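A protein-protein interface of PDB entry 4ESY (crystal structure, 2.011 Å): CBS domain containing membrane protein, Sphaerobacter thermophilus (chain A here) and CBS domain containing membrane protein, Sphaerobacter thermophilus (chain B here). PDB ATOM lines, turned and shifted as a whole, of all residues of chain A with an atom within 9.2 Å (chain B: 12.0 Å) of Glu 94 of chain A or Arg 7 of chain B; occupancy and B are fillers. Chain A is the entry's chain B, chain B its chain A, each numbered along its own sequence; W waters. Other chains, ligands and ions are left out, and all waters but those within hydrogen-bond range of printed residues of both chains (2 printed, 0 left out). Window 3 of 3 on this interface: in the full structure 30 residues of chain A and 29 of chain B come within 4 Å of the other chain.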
ATOM      1  N   SER A  74      19.615  -1.827 -12.682  1.00  0.00           N
ATOM      2  CA  SER A  74      20.468  -1.455 -11.551  1.00  0.00           C
ATOM      3  C   SER A  74      21.787  -2.200 -11.485  1.00  0.00           C
ATOM      4  O   SER A  74      22.318  -2.403 -10.397  1.00  0.00           O
ATOM      5  CB  SER A  74      19.727  -1.617 -10.212  1.00  0.00           C
ATOM      6  OG  SER A  74      18.554  -0.845 -10.219  1.00  0.00           O
ATOM      7  N   ILE A  75      22.325  -2.586 -12.643  1.00  0.00           N
ATOM      8  CA  ILE A  75      23.635  -3.226 -12.699  1.00  0.00           C
ATOM      9  C   ILE A  75      24.553  -2.339 -13.547  1.00  0.00           C
ATOM     10  O   ILE A  75      24.217  -1.990 -14.682  1.00  0.00           O
ATOM     11  CB  ILE A  75      23.561  -4.591 -13.442  1.00  0.00           C
ATOM     12  CG1 ILE A  75      22.570  -5.540 -12.771  1.00  0.00           C
ATOM     13  CG2 ILE A  75      24.922  -5.244 -13.545  1.00  0.00           C
ATOM     14  CD1 ILE A  75      22.214  -6.739 -13.687  1.00  0.00           C
ATOM     15  N   PRO A  76      25.729  -1.990 -13.005  1.00  0.00           N
ATOM     16  CA  PRO A  76      26.667  -1.226 -13.818  1.00  0.00           C
ATOM     17  C   PRO A  76      27.420  -2.227 -14.723  1.00  0.00           C
ATOM     18  O   PRO A  76      28.053  -3.174 -14.240  1.00  0.00           O
ATOM     19  CB  PRO A  76      27.614  -0.618 -12.767  1.00  0.00           C
ATOM     20  CG  PRO A  76      27.650  -1.660 -11.666  1.00  0.00           C
ATOM     21  CD  PRO A  76      26.320  -2.422 -11.722  1.00  0.00           C
ATOM     22  N   ILE A  79      30.943  -3.870 -13.945  1.00  0.00           N
ATOM     23  CA  ILE A  79      31.163  -5.008 -13.078  1.00  0.00           C
ATOM     24  C   ILE A  79      31.696  -6.236 -13.841  1.00  0.00           C
ATOM     25  O   ILE A  79      32.481  -7.034 -13.297  1.00  0.00           O
ATOM     26  CB  ILE A  79      29.900  -5.359 -12.284  1.00  0.00           C
ATOM     27  CG1 ILE A  79      30.290  -6.214 -11.121  1.00  0.00           C
ATOM     28  CG2 ILE A  79      28.824  -6.086 -13.154  1.00  0.00           C
ATOM     29  CD1 ILE A  79      29.195  -6.359 -10.151  1.00  0.00           C
ATOM     30  N   LEU A  86      36.115  -2.389  -8.801  1.00  0.00           N
ATOM     31  CA  LEU A  86      34.856  -2.040  -8.169  1.00  0.00           C
ATOM     32  C   LEU A  86      34.729  -2.533  -6.735  1.00  0.00           C
ATOM     33  O   LEU A  86      34.149  -1.836  -5.894  1.00  0.00           O
ATOM     34  CB  LEU A  86      33.677  -2.500  -9.011  1.00  0.00           C
ATOM     35  CG  LEU A  86      33.502  -1.614 -10.245  1.00  0.00           C
ATOM     36  CD1 LEU A  86      32.201  -1.950 -10.967  1.00  0.00           C
ATOM     37  CD2 LEU A  86      33.563  -0.122  -9.871  1.00  0.00           C
ATOM     38  N   SER A  87      35.321  -3.693  -6.445  1.00  0.00           N
ATOM     39  CA  SER A  87      35.350  -4.229  -5.078  1.00  0.00           C
ATOM     40  C   SER A  87      36.138  -3.405  -4.083  1.00  0.00           C
ATOM     41  O   SER A  87      35.994  -3.595  -2.886  1.00  0.00           O
ATOM     42  CB  SER A  87      35.860  -5.664  -5.061  1.00  0.00           C
ATOM     43  OG  SER A  87      35.052  -6.451  -5.922  1.00  0.00           O
ATOM     44  N   ALA A  89      35.566  -0.362  -3.948  1.00  0.00           N
ATOM     45  CA  ALA A  89      34.531   0.628  -3.671  1.00  0.00           C
ATOM     46  C   ALA A  89      33.304   0.036  -2.970  1.00  0.00           C
ATOM     47  O   ALA A  89      32.636   0.704  -2.207  1.00  0.00           O
ATOM     48  CB  ALA A  89      34.106   1.300  -4.969  1.00  0.00           C
ATOM     49  N   ILE A  90      33.017  -1.223  -3.267  1.00  0.00           N
ATOM     50  CA  ILE A  90      31.759  -1.873  -2.925  1.00  0.00           C
ATOM     51  C   ILE A  90      32.093  -3.161  -2.171  1.00  0.00           C
ATOM     52  O   ILE A  90      32.890  -3.971  -2.652  1.00  0.00           O
ATOM     53  CB  ILE A  90      31.015  -2.230  -4.230  1.00  0.00           C
ATOM     54  CG1 ILE A  90      30.820  -0.967  -5.089  1.00  0.00           C
ATOM     55  CG2 ILE A  90      29.696  -2.882  -3.950  1.00  0.00           C
ATOM     56  CD1 ILE A  90      30.147  -1.194  -6.445  1.00  0.00           C
ATOM     57  N   PRO A  91      31.489  -3.362  -0.990  1.00  0.00           N
ATOM     58  CA  PRO A  91      31.763  -4.608  -0.262  1.00  0.00           C
ATOM     59  C   PRO A  91      31.415  -5.858  -1.105  1.00  0.00           C
ATOM     60  O   PRO A  91      30.558  -5.803  -2.003  1.00  0.00           O
ATOM     61  CB  PRO A  91      30.897  -4.494   1.005  1.00  0.00           C
ATOM     62  CG  PRO A  91      29.851  -3.476   0.680  1.00  0.00           C
ATOM     63  CD  PRO A  91      30.432  -2.549  -0.362  1.00  0.00           C
ATOM     64  N   ALA A  92      32.141  -6.947  -0.860  1.00  0.00           N
ATOM     65  CA  ALA A  92      31.970  -8.191  -1.619  1.00  0.00           C
ATOM     66  C   ALA A  92      30.552  -8.786  -1.638  1.00  0.00           C
ATOM     67  O   ALA A  92      30.136  -9.294  -2.665  1.00  0.00           O
ATOM     68  CB  ALA A  92      32.993  -9.256  -1.182  1.00  0.00           C
ATOM     69  N   PRO A  93      29.810  -8.744  -0.510  1.00  0.00           N
ATOM     70  CA  PRO A  93      28.452  -9.296  -0.650  1.00  0.00           C
ATOM     71  C   PRO A  93      27.592  -8.485  -1.632  1.00  0.00           C
ATOM     72  O   PRO A  93      26.721  -9.045  -2.285  1.00  0.00           O
ATOM     73  CB  PRO A  93      27.874  -9.191   0.770  1.00  0.00           C
ATOM     74  CG  PRO A  93      29.052  -9.098   1.664  1.00  0.00           C
ATOM     75  CD  PRO A  93      30.109  -8.370   0.883  1.00  0.00           C
ATOM     76  N   GLU A  94      27.855  -7.186  -1.747  1.00  0.00           N
ATOM     77  CA  GLU A  94      27.062  -6.344  -2.628  1.00  0.00           C
ATOM     78  C   GLU A  94      27.418  -6.569  -4.092  1.00  0.00           C
ATOM     79  O   GLU A  94      26.545  -6.534  -4.948  1.00  0.00           O
ATOM     80  CB  GLU A  94      27.205  -4.865  -2.255  1.00  0.00           C
ATOM     81  CG  GLU A  94      26.655  -4.545  -0.878  1.00  0.00           C
ATOM     82  CD  GLU A  94      25.258  -5.118  -0.692  1.00  0.00           C
ATOM     83  OE1 GLU A  94      24.361  -4.799  -1.515  1.00  0.00           O
ATOM     84  OE2 GLU A  94      25.071  -5.916   0.255  1.00  0.00           O
ATOM     85  N   VAL A  95      28.703  -6.764  -4.381  1.00  0.00           N
ATOM     86  CA  VAL A  95      29.132  -7.114  -5.742  1.00  0.00           C
ATOM     87  C   VAL A  95      28.532  -8.460  -6.118  1.00  0.00           C
ATOM     88  O   VAL A  95      28.084  -8.655  -7.237  1.00  0.00           O
ATOM     89  CB  VAL A  95      30.692  -7.205  -5.860  1.00  0.00           C
ATOM     90  CG1 VAL A  95      31.114  -7.728  -7.260  1.00  0.00           C
ATOM     91  CG2 VAL A  95      31.355  -5.866  -5.527  1.00  0.00           C
ATOM     92  N   GLU A  96      28.537  -9.405  -5.184  1.00  0.00           N
ATOM     93  CA  GLU A  96      27.996 -10.715  -5.498  1.00  0.00           C
ATOM     94  C   GLU A  96      26.514 -10.622  -5.805  1.00  0.00           C
ATOM     95  O   GLU A  96      26.009 -11.308  -6.699  1.00  0.00           O
ATOM     96  CB  GLU A  96      28.248 -11.713  -4.375  1.00  0.00           C
ATOM     97  CG  GLU A  96      29.052 -12.927  -4.835  1.00  0.00           C
ATOM     98  CD  GLU A  96      28.527 -13.585  -6.136  1.00  0.00           C
ATOM     99  OE1 GLU A  96      29.356 -13.831  -7.049  1.00  0.00           O
ATOM    100  OE2 GLU A  96      27.307 -13.878  -6.245  1.00  0.00           O
ATOM    101  N   HIS A  97      25.829  -9.740  -5.092  1.00  0.00           N
ATOM    102  CA  HIS A  97      24.409  -9.515  -5.336  1.00  0.00           C
ATOM    103  C   HIS A  97      24.135  -8.945  -6.747  1.00  0.00           C
ATOM    104  O   HIS A  97      23.135  -9.288  -7.418  1.00  0.00           O
ATOM    105  CB  HIS A  97      23.840  -8.599  -4.259  1.00  0.00           C
ATOM    106  CG  HIS A  97      22.397  -8.278  -4.464  1.00  0.00           C
ATOM    107  ND1 HIS A  97      21.410  -9.236  -4.400  1.00  0.00           N
ATOM    108  CD2 HIS A  97      21.781  -7.116  -4.791  1.00  0.00           C
ATOM    109  CE1 HIS A  97      20.242  -8.673  -4.655  1.00  0.00           C
ATOM    110  NE2 HIS A  97      20.440  -7.389  -4.900  1.00  0.00           N
ATOM    111  N   LEU A  98      25.026  -8.067  -7.194  1.00  0.00           N
ATOM    112  CA  LEU A  98      24.963  -7.579  -8.561  1.00  0.00           C
ATOM    113  C   LEU A  98      25.103  -8.718  -9.569  1.00  0.00           C
ATOM    114  O   LEU A  98      24.319  -8.819 -10.511  1.00  0.00           O
ATOM    115  CB  LEU A  98      26.035  -6.506  -8.791  1.00  0.00           C
ATOM    116  CG  LEU A  98      25.806  -5.231  -7.981  1.00  0.00           C
ATOM    117  CD1 LEU A  98      26.916  -4.212  -8.281  1.00  0.00           C
ATOM    118  CD2 LEU A  98      24.410  -4.657  -8.279  1.00  0.00           C
ATOM    119  N   PHE A  99      26.105  -9.562  -9.390  1.00  0.00           N
ATOM    120  CA  PHE A  99      26.250 -10.741 -10.246  1.00  0.00           C
ATOM    121  C   PHE A  99      25.017 -11.657 -10.232  1.00  0.00           C
ATOM    122  O   PHE A  99      24.613 -12.169 -11.290  1.00  0.00           O
ATOM    123  CB  PHE A  99      27.504 -11.546  -9.904  1.00  0.00           C
ATOM    124  CG  PHE A  99      28.778 -10.911 -10.380  1.00  0.00           C
ATOM    125  CD1 PHE A  99      28.907 -10.472 -11.693  1.00  0.00           C
ATOM    126  CD2 PHE A  99      29.848 -10.725  -9.499  1.00  0.00           C
ATOM    127  CE1 PHE A  99      30.104  -9.874 -12.138  1.00  0.00           C
ATOM    128  CE2 PHE A  99      31.048 -10.130  -9.926  1.00  0.00           C
ATOM    129  CZ  PHE A  99      31.179  -9.706 -11.244  1.00  0.00           C
ATOM    130  N   GLU A 100      24.450 -11.863  -9.045  1.00  0.00           N
ATOM    131  CA  GLU A 100      23.252 -12.687  -8.879  1.00  0.00           C
ATOM    132  C   GLU A 100      22.111 -12.113  -9.741  1.00  0.00           C
ATOM    133  O   GLU A 100      21.433 -12.826 -10.479  1.00  0.00           O
ATOM    134  CB  GLU A 100      22.835 -12.736  -7.393  1.00  0.00           C
ATOM    135  CG  GLU A 100      23.831 -13.418  -6.458  1.00  0.00           C
ATOM    136  CD  GLU A 100      23.546 -13.186  -4.946  1.00  0.00           C
ATOM    137  OE1 GLU A 100      24.378 -13.603  -4.102  1.00  0.00           O
ATOM    138  OE2 GLU A 100      22.502 -12.587  -4.595  1.00  0.00           O
ATOM    139  N   THR A 101      21.917 -10.807  -9.645  1.00  0.00           N
ATOM    140  CA  THR A 101      20.895 -10.116 -10.406  1.00  0.00           C
ATOM    141  C   THR A 101      21.125 -10.272 -11.914  1.00  0.00           C
ATOM    142  O   THR A 101      20.177 -10.470 -12.664  1.00  0.00           O
ATOM    143  CB  THR A 101      20.842  -8.625 -10.020  1.00  0.00           C
ATOM    144  OG1 THR A 101      20.419  -8.518  -8.648  1.00  0.00           O
ATOM    145  CG2 THR A 101      19.822  -7.877 -10.903  1.00  0.00           C
ATOM    146  N   ARG B   1      11.358  -4.154  -0.424  1.00  0.00           N
ATOM    147  CA  ARG B   1      11.307  -3.087  -1.417  1.00  0.00           C
ATOM    148  C   ARG B   1      12.102  -1.877  -0.953  1.00  0.00           C
ATOM    149  O   ARG B   1      12.847  -1.270  -1.730  1.00  0.00           O
ATOM    150  CB  ARG B   1       9.868  -2.648  -1.669  1.00  0.00           C
ATOM    151  CG  ARG B   1       8.942  -3.722  -2.199  1.00  0.00           C
ATOM    152  CD  ARG B   1       7.563  -3.124  -2.427  1.00  0.00           C
ATOM    153  NE  ARG B   1       6.652  -4.030  -3.115  1.00  0.00           N
ATOM    154  CZ  ARG B   1       5.444  -3.675  -3.536  1.00  0.00           C
ATOM    155  NH1 ARG B   1       5.017  -2.433  -3.343  1.00  0.00           N
ATOM    156  NH2 ARG B   1       4.662  -4.555  -4.151  1.00  0.00           N
ATOM    157  N   VAL B   2      11.920  -1.518   0.315  1.00  0.00           N
ATOM    158  CA  VAL B   2      12.625  -0.373   0.893  1.00  0.00           C
ATOM    159  C   VAL B   2      14.120  -0.681   1.021  1.00  0.00           C
ATOM    160  O   VAL B   2      14.974   0.170   0.717  1.00  0.00           O
ATOM    161  CB  VAL B   2      11.997   0.071   2.267  1.00  0.00           C
ATOM    162  CG1 VAL B   2      12.276  -0.944   3.387  1.00  0.00           C
ATOM    163  CG2 VAL B   2      12.469   1.467   2.666  1.00  0.00           C
ATOM    164  N   ALA B   3      14.419  -1.911   1.450  1.00  0.00           N
ATOM    165  CA  ALA B   3      15.783  -2.364   1.688  1.00  0.00           C
ATOM    166  C   ALA B   3      16.522  -2.460   0.365  1.00  0.00           C
ATOM    167  O   ALA B   3      17.709  -2.118   0.279  1.00  0.00           O
ATOM    168  CB  ALA B   3      15.778  -3.711   2.390  1.00  0.00           C
ATOM    169  N   GLU B   4      15.811  -2.926  -0.663  1.00  0.00           N
ATOM    170  CA  GLU B   4      16.377  -2.961  -1.998  1.00  0.00           C
ATOM    171  C   GLU B   4      16.793  -1.567  -2.446  1.00  0.00           C
ATOM    172  O   GLU B   4      17.869  -1.398  -3.014  1.00  0.00           O
ATOM    173  CB  GLU B   4      15.410  -3.563  -3.012  1.00  0.00           C
ATOM    174  CG  GLU B   4      16.097  -3.813  -4.342  1.00  0.00           C
ATOM    175  CD  GLU B   4      17.271  -4.772  -4.198  1.00  0.00           C
ATOM    176  OE1 GLU B   4      17.121  -5.808  -3.502  1.00  0.00           O
ATOM    177  OE2 GLU B   4      18.340  -4.496  -4.770  1.00  0.00           O
ATOM    178  N   GLN B   5      15.948  -0.573  -2.181  1.00  0.00           N
ATOM    179  CA  GLN B   5      16.298   0.821  -2.477  1.00  0.00           C
ATOM    180  C   GLN B   5      17.513   1.342  -1.707  1.00  0.00           C
ATOM    181  O   GLN B   5      18.374   2.004  -2.284  1.00  0.00           O
ATOM    182  CB  GLN B   5      15.111   1.768  -2.276  1.00  0.00           C
ATOM    183  CG  GLN B   5      14.197   1.878  -3.489  1.00  0.00           C
ATOM    184  CD  GLN B   5      14.935   1.700  -4.814  1.00  0.00           C
ATOM    185  OE1 GLN B   5      14.642   0.765  -5.574  1.00  0.00           O
ATOM    186  NE2 GLN B   5      15.887   2.602  -5.107  1.00  0.00           N
ATOM    187  N   ALA B   6      17.569   1.055  -0.411  1.00  0.00           N
ATOM    188  CA  ALA B   6      18.740   1.425   0.369  1.00  0.00           C
ATOM    189  C   ALA B   6      19.994   0.782  -0.207  1.00  0.00           C
ATOM    190  O   ALA B   6      21.055   1.384  -0.243  1.00  0.00           O
ATOM    191  CB  ALA B   6      18.558   1.029   1.819  1.00  0.00           C
ATOM    192  N   ARG B   7      19.849  -0.452  -0.662  1.00  0.00           N
ATOM    193  CA  ARG B   7      20.941  -1.208  -1.240  1.00  0.00           C
ATOM    194  C   ARG B   7      21.448  -0.528  -2.524  1.00  0.00           C
ATOM    195  O   ARG B   7      22.660  -0.364  -2.731  1.00  0.00           O
ATOM    196  CB  ARG B   7      20.447  -2.626  -1.518  1.00  0.00           C
ATOM    197  CG  ARG B   7      21.515  -3.659  -1.600  1.00  0.00           C
ATOM    198  CD  ARG B   7      20.888  -5.048  -1.515  1.00  0.00           C
ATOM    199  NE  ARG B   7      21.904  -6.091  -1.468  1.00  0.00           N
ATOM    200  CZ  ARG B   7      21.645  -7.381  -1.276  1.00  0.00           C
ATOM    201  NH1 ARG B   7      20.391  -7.806  -1.112  1.00  0.00           N
ATOM    202  NH2 ARG B   7      22.652  -8.248  -1.255  1.00  0.00           N
ATOM    203  N   ARG B   8      20.501  -0.106  -3.358  1.00  0.00           N
ATOM    204  CA  ARG B   8      20.792   0.544  -4.634  1.00  0.00           C
ATOM    205  C   ARG B   8      21.407   1.931  -4.427  1.00  0.00           C
ATOM    206  O   ARG B   8      22.286   2.367  -5.180  1.00  0.00           O
ATOM    207  CB  ARG B   8      19.511   0.646  -5.482  1.00  0.00           C
ATOM    208  CG  ARG B   8      19.190  -0.624  -6.275  1.00  0.00           C
ATOM    209  CD  ARG B   8      17.762  -0.645  -6.761  1.00  0.00           C
ATOM    210  NE  ARG B   8      17.515  -1.834  -7.582  1.00  0.00           N
ATOM    211  CZ  ARG B   8      16.314  -2.263  -7.962  1.00  0.00           C
ATOM    212  NH1 ARG B   8      15.222  -1.602  -7.587  1.00  0.00           N
ATOM    213  NH2 ARG B   8      16.204  -3.364  -8.708  1.00  0.00           N
ATOM    214  N   ARG B   9      20.933   2.603  -3.389  1.00  0.00           N
ATOM    215  CA  ARG B   9      21.397   3.931  -3.062  1.00  0.00           C
ATOM    216  C   ARG B   9      22.870   3.865  -2.670  1.00  0.00           C
ATOM    217  O   ARG B   9      23.684   4.675  -3.143  1.00  0.00           O
ATOM    218  CB  ARG B   9      20.543   4.500  -1.917  1.00  0.00           C
ATOM    219  CG  ARG B   9      20.723   5.956  -1.676  1.00  0.00           C
ATOM    220  CD  ARG B   9      19.642   6.548  -0.777  1.00  0.00           C
ATOM    221  NE  ARG B   9      19.580   5.952   0.561  1.00  0.00           N
ATOM    222  CZ  ARG B   9      18.572   5.196   0.994  1.00  0.00           C
ATOM    223  NH1 ARG B   9      18.593   4.688   2.230  1.00  0.00           N
ATOM    224  NH2 ARG B   9      17.533   4.952   0.191  1.00  0.00           N
ATOM    225  N   ALA B  10      23.220   2.903  -1.815  1.00  0.00           N
ATOM    226  CA  ALA B  10      24.608   2.781  -1.364  1.00  0.00           C
ATOM    227  C   ALA B  10      25.575   2.432  -2.509  1.00  0.00           C
ATOM    228  O   ALA B  10      26.663   3.001  -2.599  1.00  0.00           O
ATOM    229  CB  ALA B  10      24.725   1.760  -0.203  1.00  0.00           C
ATOM    230  N   ILE B  11      25.183   1.514  -3.393  1.00  0.00           N
ATOM    231  CA  ILE B  11      25.985   1.212  -4.581  1.00  0.00           C
ATOM    232  C   ILE B  11      26.183   2.462  -5.454  1.00  0.00           C
ATOM    233  O   ILE B  11      27.290   2.765  -5.864  1.00  0.00           O
ATOM    234  CB  ILE B  11      25.318   0.153  -5.449  1.00  0.00           C
ATOM    235  CG1 ILE B  11      25.005  -1.096  -4.630  1.00  0.00           C
ATOM    236  CG2 ILE B  11      26.178  -0.188  -6.682  1.00  0.00           C
ATOM    237  CD1 ILE B  11      26.196  -1.843  -4.169  1.00  0.00           C
ATOM    238  N   ALA B  12      25.109   3.200  -5.725  1.00  0.00           N
ATOM    239  CA  ALA B  12      25.220   4.401  -6.554  1.00  0.00           C
ATOM    240  C   ALA B  12      26.166   5.427  -5.941  1.00  0.00           C
ATOM    241  O   ALA B  12      26.969   6.039  -6.656  1.00  0.00           O
ATOM    242  CB  ALA B  12      23.849   5.031  -6.828  1.00  0.00           C
ATOM    243  N   ARG B  13      26.081   5.615  -4.628  1.00  0.00           N
ATOM    244  CA  ARG B  13      26.968   6.563  -3.962  1.00  0.00           C
ATOM    245  C   ARG B  13      28.428   6.128  -4.007  1.00  0.00           C
ATOM    246  O   ARG B  13      29.314   6.943  -4.244  1.00  0.00           O
ATOM    247  CB  ARG B  13      26.537   6.805  -2.506  1.00  0.00           C
ATOM    248  CG  ARG B  13      25.167   7.430  -2.365  1.00  0.00           C
ATOM    249  CD  ARG B  13      24.904   7.803  -0.911  1.00  0.00           C
ATOM    250  NE  ARG B  13      25.910   8.748  -0.470  1.00  0.00           N
ATOM    251  CZ  ARG B  13      25.881  10.049  -0.743  1.00  0.00           C
ATOM    252  NH1 ARG B  13      26.864  10.806  -0.291  1.00  0.00           N
ATOM    253  NH2 ARG B  13      24.878  10.594  -1.444  1.00  0.00           N
ATOM    254  N   ALA B  14      28.666   4.850  -3.754  1.00  0.00           N
ATOM    255  CA  ALA B  14      29.995   4.259  -3.859  1.00  0.00           C
ATOM    256  C   ALA B  14      30.603   4.469  -5.246  1.00  0.00           C
ATOM    257  O   ALA B  14      31.791   4.790  -5.404  1.00  0.00           O
ATOM    258  CB  ALA B  14      29.889   2.754  -3.582  1.00  0.00           C
ATOM    259  N   ILE B  15      29.771   4.301  -6.259  1.00  0.00           N
ATOM    260  CA  ILE B  15      30.253   4.431  -7.622  1.00  0.00           C
ATOM    261  C   ILE B  15      30.633   5.876  -7.918  1.00  0.00           C
ATOM    262  O   ILE B  15      31.640   6.098  -8.546  1.00  0.00           O
ATOM    263  CB  ILE B  15      29.241   3.866  -8.628  1.00  0.00           C
ATOM    264  CG1 ILE B  15      29.306   2.336  -8.571  1.00  0.00           C
ATOM    265  CG2 ILE B  15      29.543   4.348 -10.041  1.00  0.00           C
ATOM    266  CD1 ILE B  15      28.250   1.635  -9.404  1.00  0.00           C
ATOM    267  N   ARG B  16      29.873   6.858  -7.414  1.00  0.00           N
ATOM    268  CA  ARG B  16      30.247   8.250  -7.639  1.00  0.00           C
ATOM    269  C   ARG B  16      31.573   8.624  -6.952  1.00  0.00           C
ATOM    270  O   ARG B  16      32.222   9.595  -7.361  1.00  0.00           O
ATOM    271  CB  ARG B  16      29.145   9.218  -7.198  1.00  0.00           C
ATOM    272  CG  ARG B  16      27.944   9.298  -8.131  1.00  0.00           C
ATOM    273  CD  ARG B  16      26.896  10.289  -7.591  1.00  0.00           C
ATOM    274  NE  ARG B  16      27.486  11.618  -7.390  1.00  0.00           N
ATOM    275  CZ  ARG B  16      27.537  12.576  -8.317  1.00  0.00           C
ATOM    276  NH1 ARG B  16      28.097  13.749  -8.026  1.00  0.00           N
ATOM    277  NH2 ARG B  16      27.002  12.375  -9.519  1.00  0.00           N
ATOM    278  N   LEU B 159      28.927   2.809 -15.707  1.00  0.00           N
ATOM    279  CA  LEU B 159      28.858   2.997 -14.258  1.00  0.00           C
ATOM    280  C   LEU B 159      27.609   3.655 -13.733  1.00  0.00           C
ATOM    281  O   LEU B 159      27.125   3.292 -12.664  1.00  0.00           O
ATOM    282  CB  LEU B 159      30.013   3.915 -13.836  1.00  0.00           C
ATOM    283  CG  LEU B 159      31.377   3.312 -14.083  1.00  0.00           C
ATOM    284  CD1 LEU B 159      32.422   4.412 -13.924  1.00  0.00           C
ATOM    285  CD2 LEU B 159      31.548   2.236 -13.062  1.00  0.00           C
HETATM  286  O   HOH W   1      24.582  -1.997  -1.474  1.00  0.00           O
HETATM  287  O   HOH W   2      16.326  -1.841 -11.590  1.00  0.00           O
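OE2 of Glu 4 of chain B is in salt-bridge range of NE of Arg 8 of chain B (3.96 Å). The side-chain amide oxygen of Gln 5 of chain B lies within hydrogen-bond range of the guanidinium group of Arg 8 of chain B. The backbone carbonyl oxygen (O) of His 97 of chain A is in hydrogen-bond range of the side-chain hydroxyl (OG1) of Thr 101 of chain A.
The guanidinium group of Arg 7 of chain B lies within salt-bridge range of the side-chain carboxylate of Glu 94 of chain A, 2.8 Å away. The guanidinium group (NE) of Arg 8 of chain B lies within hydrogen-bond range of the side-chain hydroxyl (OG) of Ser 74 of chain A (3.0 Å).
Water W2 lies within hydrogen-bond range of OG of Ser 74 of chain A and NH2 of Arg 8 of chain B. Water W1 lies within hydrogen-bond range of OE1 of Glu 94 of chain A (2.8 Å) and O of Arg 7 of chain B (2.8 Å).
Among the printed residues, merely in contact across the chains: Pro 76 of chain A with Leu 159 of chain B, Ala 89 of chain A with Ala 14 of chain B, Ile 90 of chain A with Ile 11 of chain B, Glu 94 of chain A with Ile 11 of chain B, His 97 of chain A with Glu 4 of chain B and His 97 of chain A with Arg 7 of chain B.
Of the printed residues of chain B, Glu 94 of chain A touches Arg 7 and Ile 11. Printed residues of chain A within 4 Å of Arg 7 of chain B: Glu 94 and His 97. Ile 90 of chain A touches just one residue of chain B: Ile 11 (3.7 Å). No residue of chain B comes within 4 Å of Pro 91 of chain A. No residue of chain B comes within 4 Å of Ala 92 of chain A. No residue of chain B comes within 4 Å of Pro 93 of chain A. Of chain B, only Glu 4 and Arg 7 come within 4 Å of His 97 of chain A. No residue of chain B comes within 4 Å of Leu 98 of chain A. No residue of chain A comes within 4 Å of Ala 6 of chain B. Of the printed residues of chain B, Ser 74 of chain A touches Arg 8 (3.0 Å). Printed residues of chain B within 4 Å of Ala 89 of chain A: Ala 14. Ala 10 of chain B touches none of the printed residues of chain A. Phe 99 of chain A touches none of the printed residues of chain B. The nearest residue of chain B that does not touch Glu 94 of chain A is Arg 8 of chain B (6.3 Å). The nearest printed residue of chain A that does not touch Ala 14 of chain B is Ile 90 of chain A (4.1 Å).
Hydrophobic or aromatic side chains of chain B that line the printed part of chain A: Ile 11 and Ala 14. Of the 19 printed residues of chain A, 6 touch a printed residue of chain B. Printed residues of chain A that touch a printed residue of chain B: Ser 74, Pro 76, Ala 89, Ile 90, Glu 94 and His 97. Among the printed residues, 8 pairs touch across the chains. Among the printed residues, Asp or Glu carboxylates within 4 Å of a Lys or Arg side-chain nitrogen of the other chain: Glu 94 of chain A with Arg 7 of chain B.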
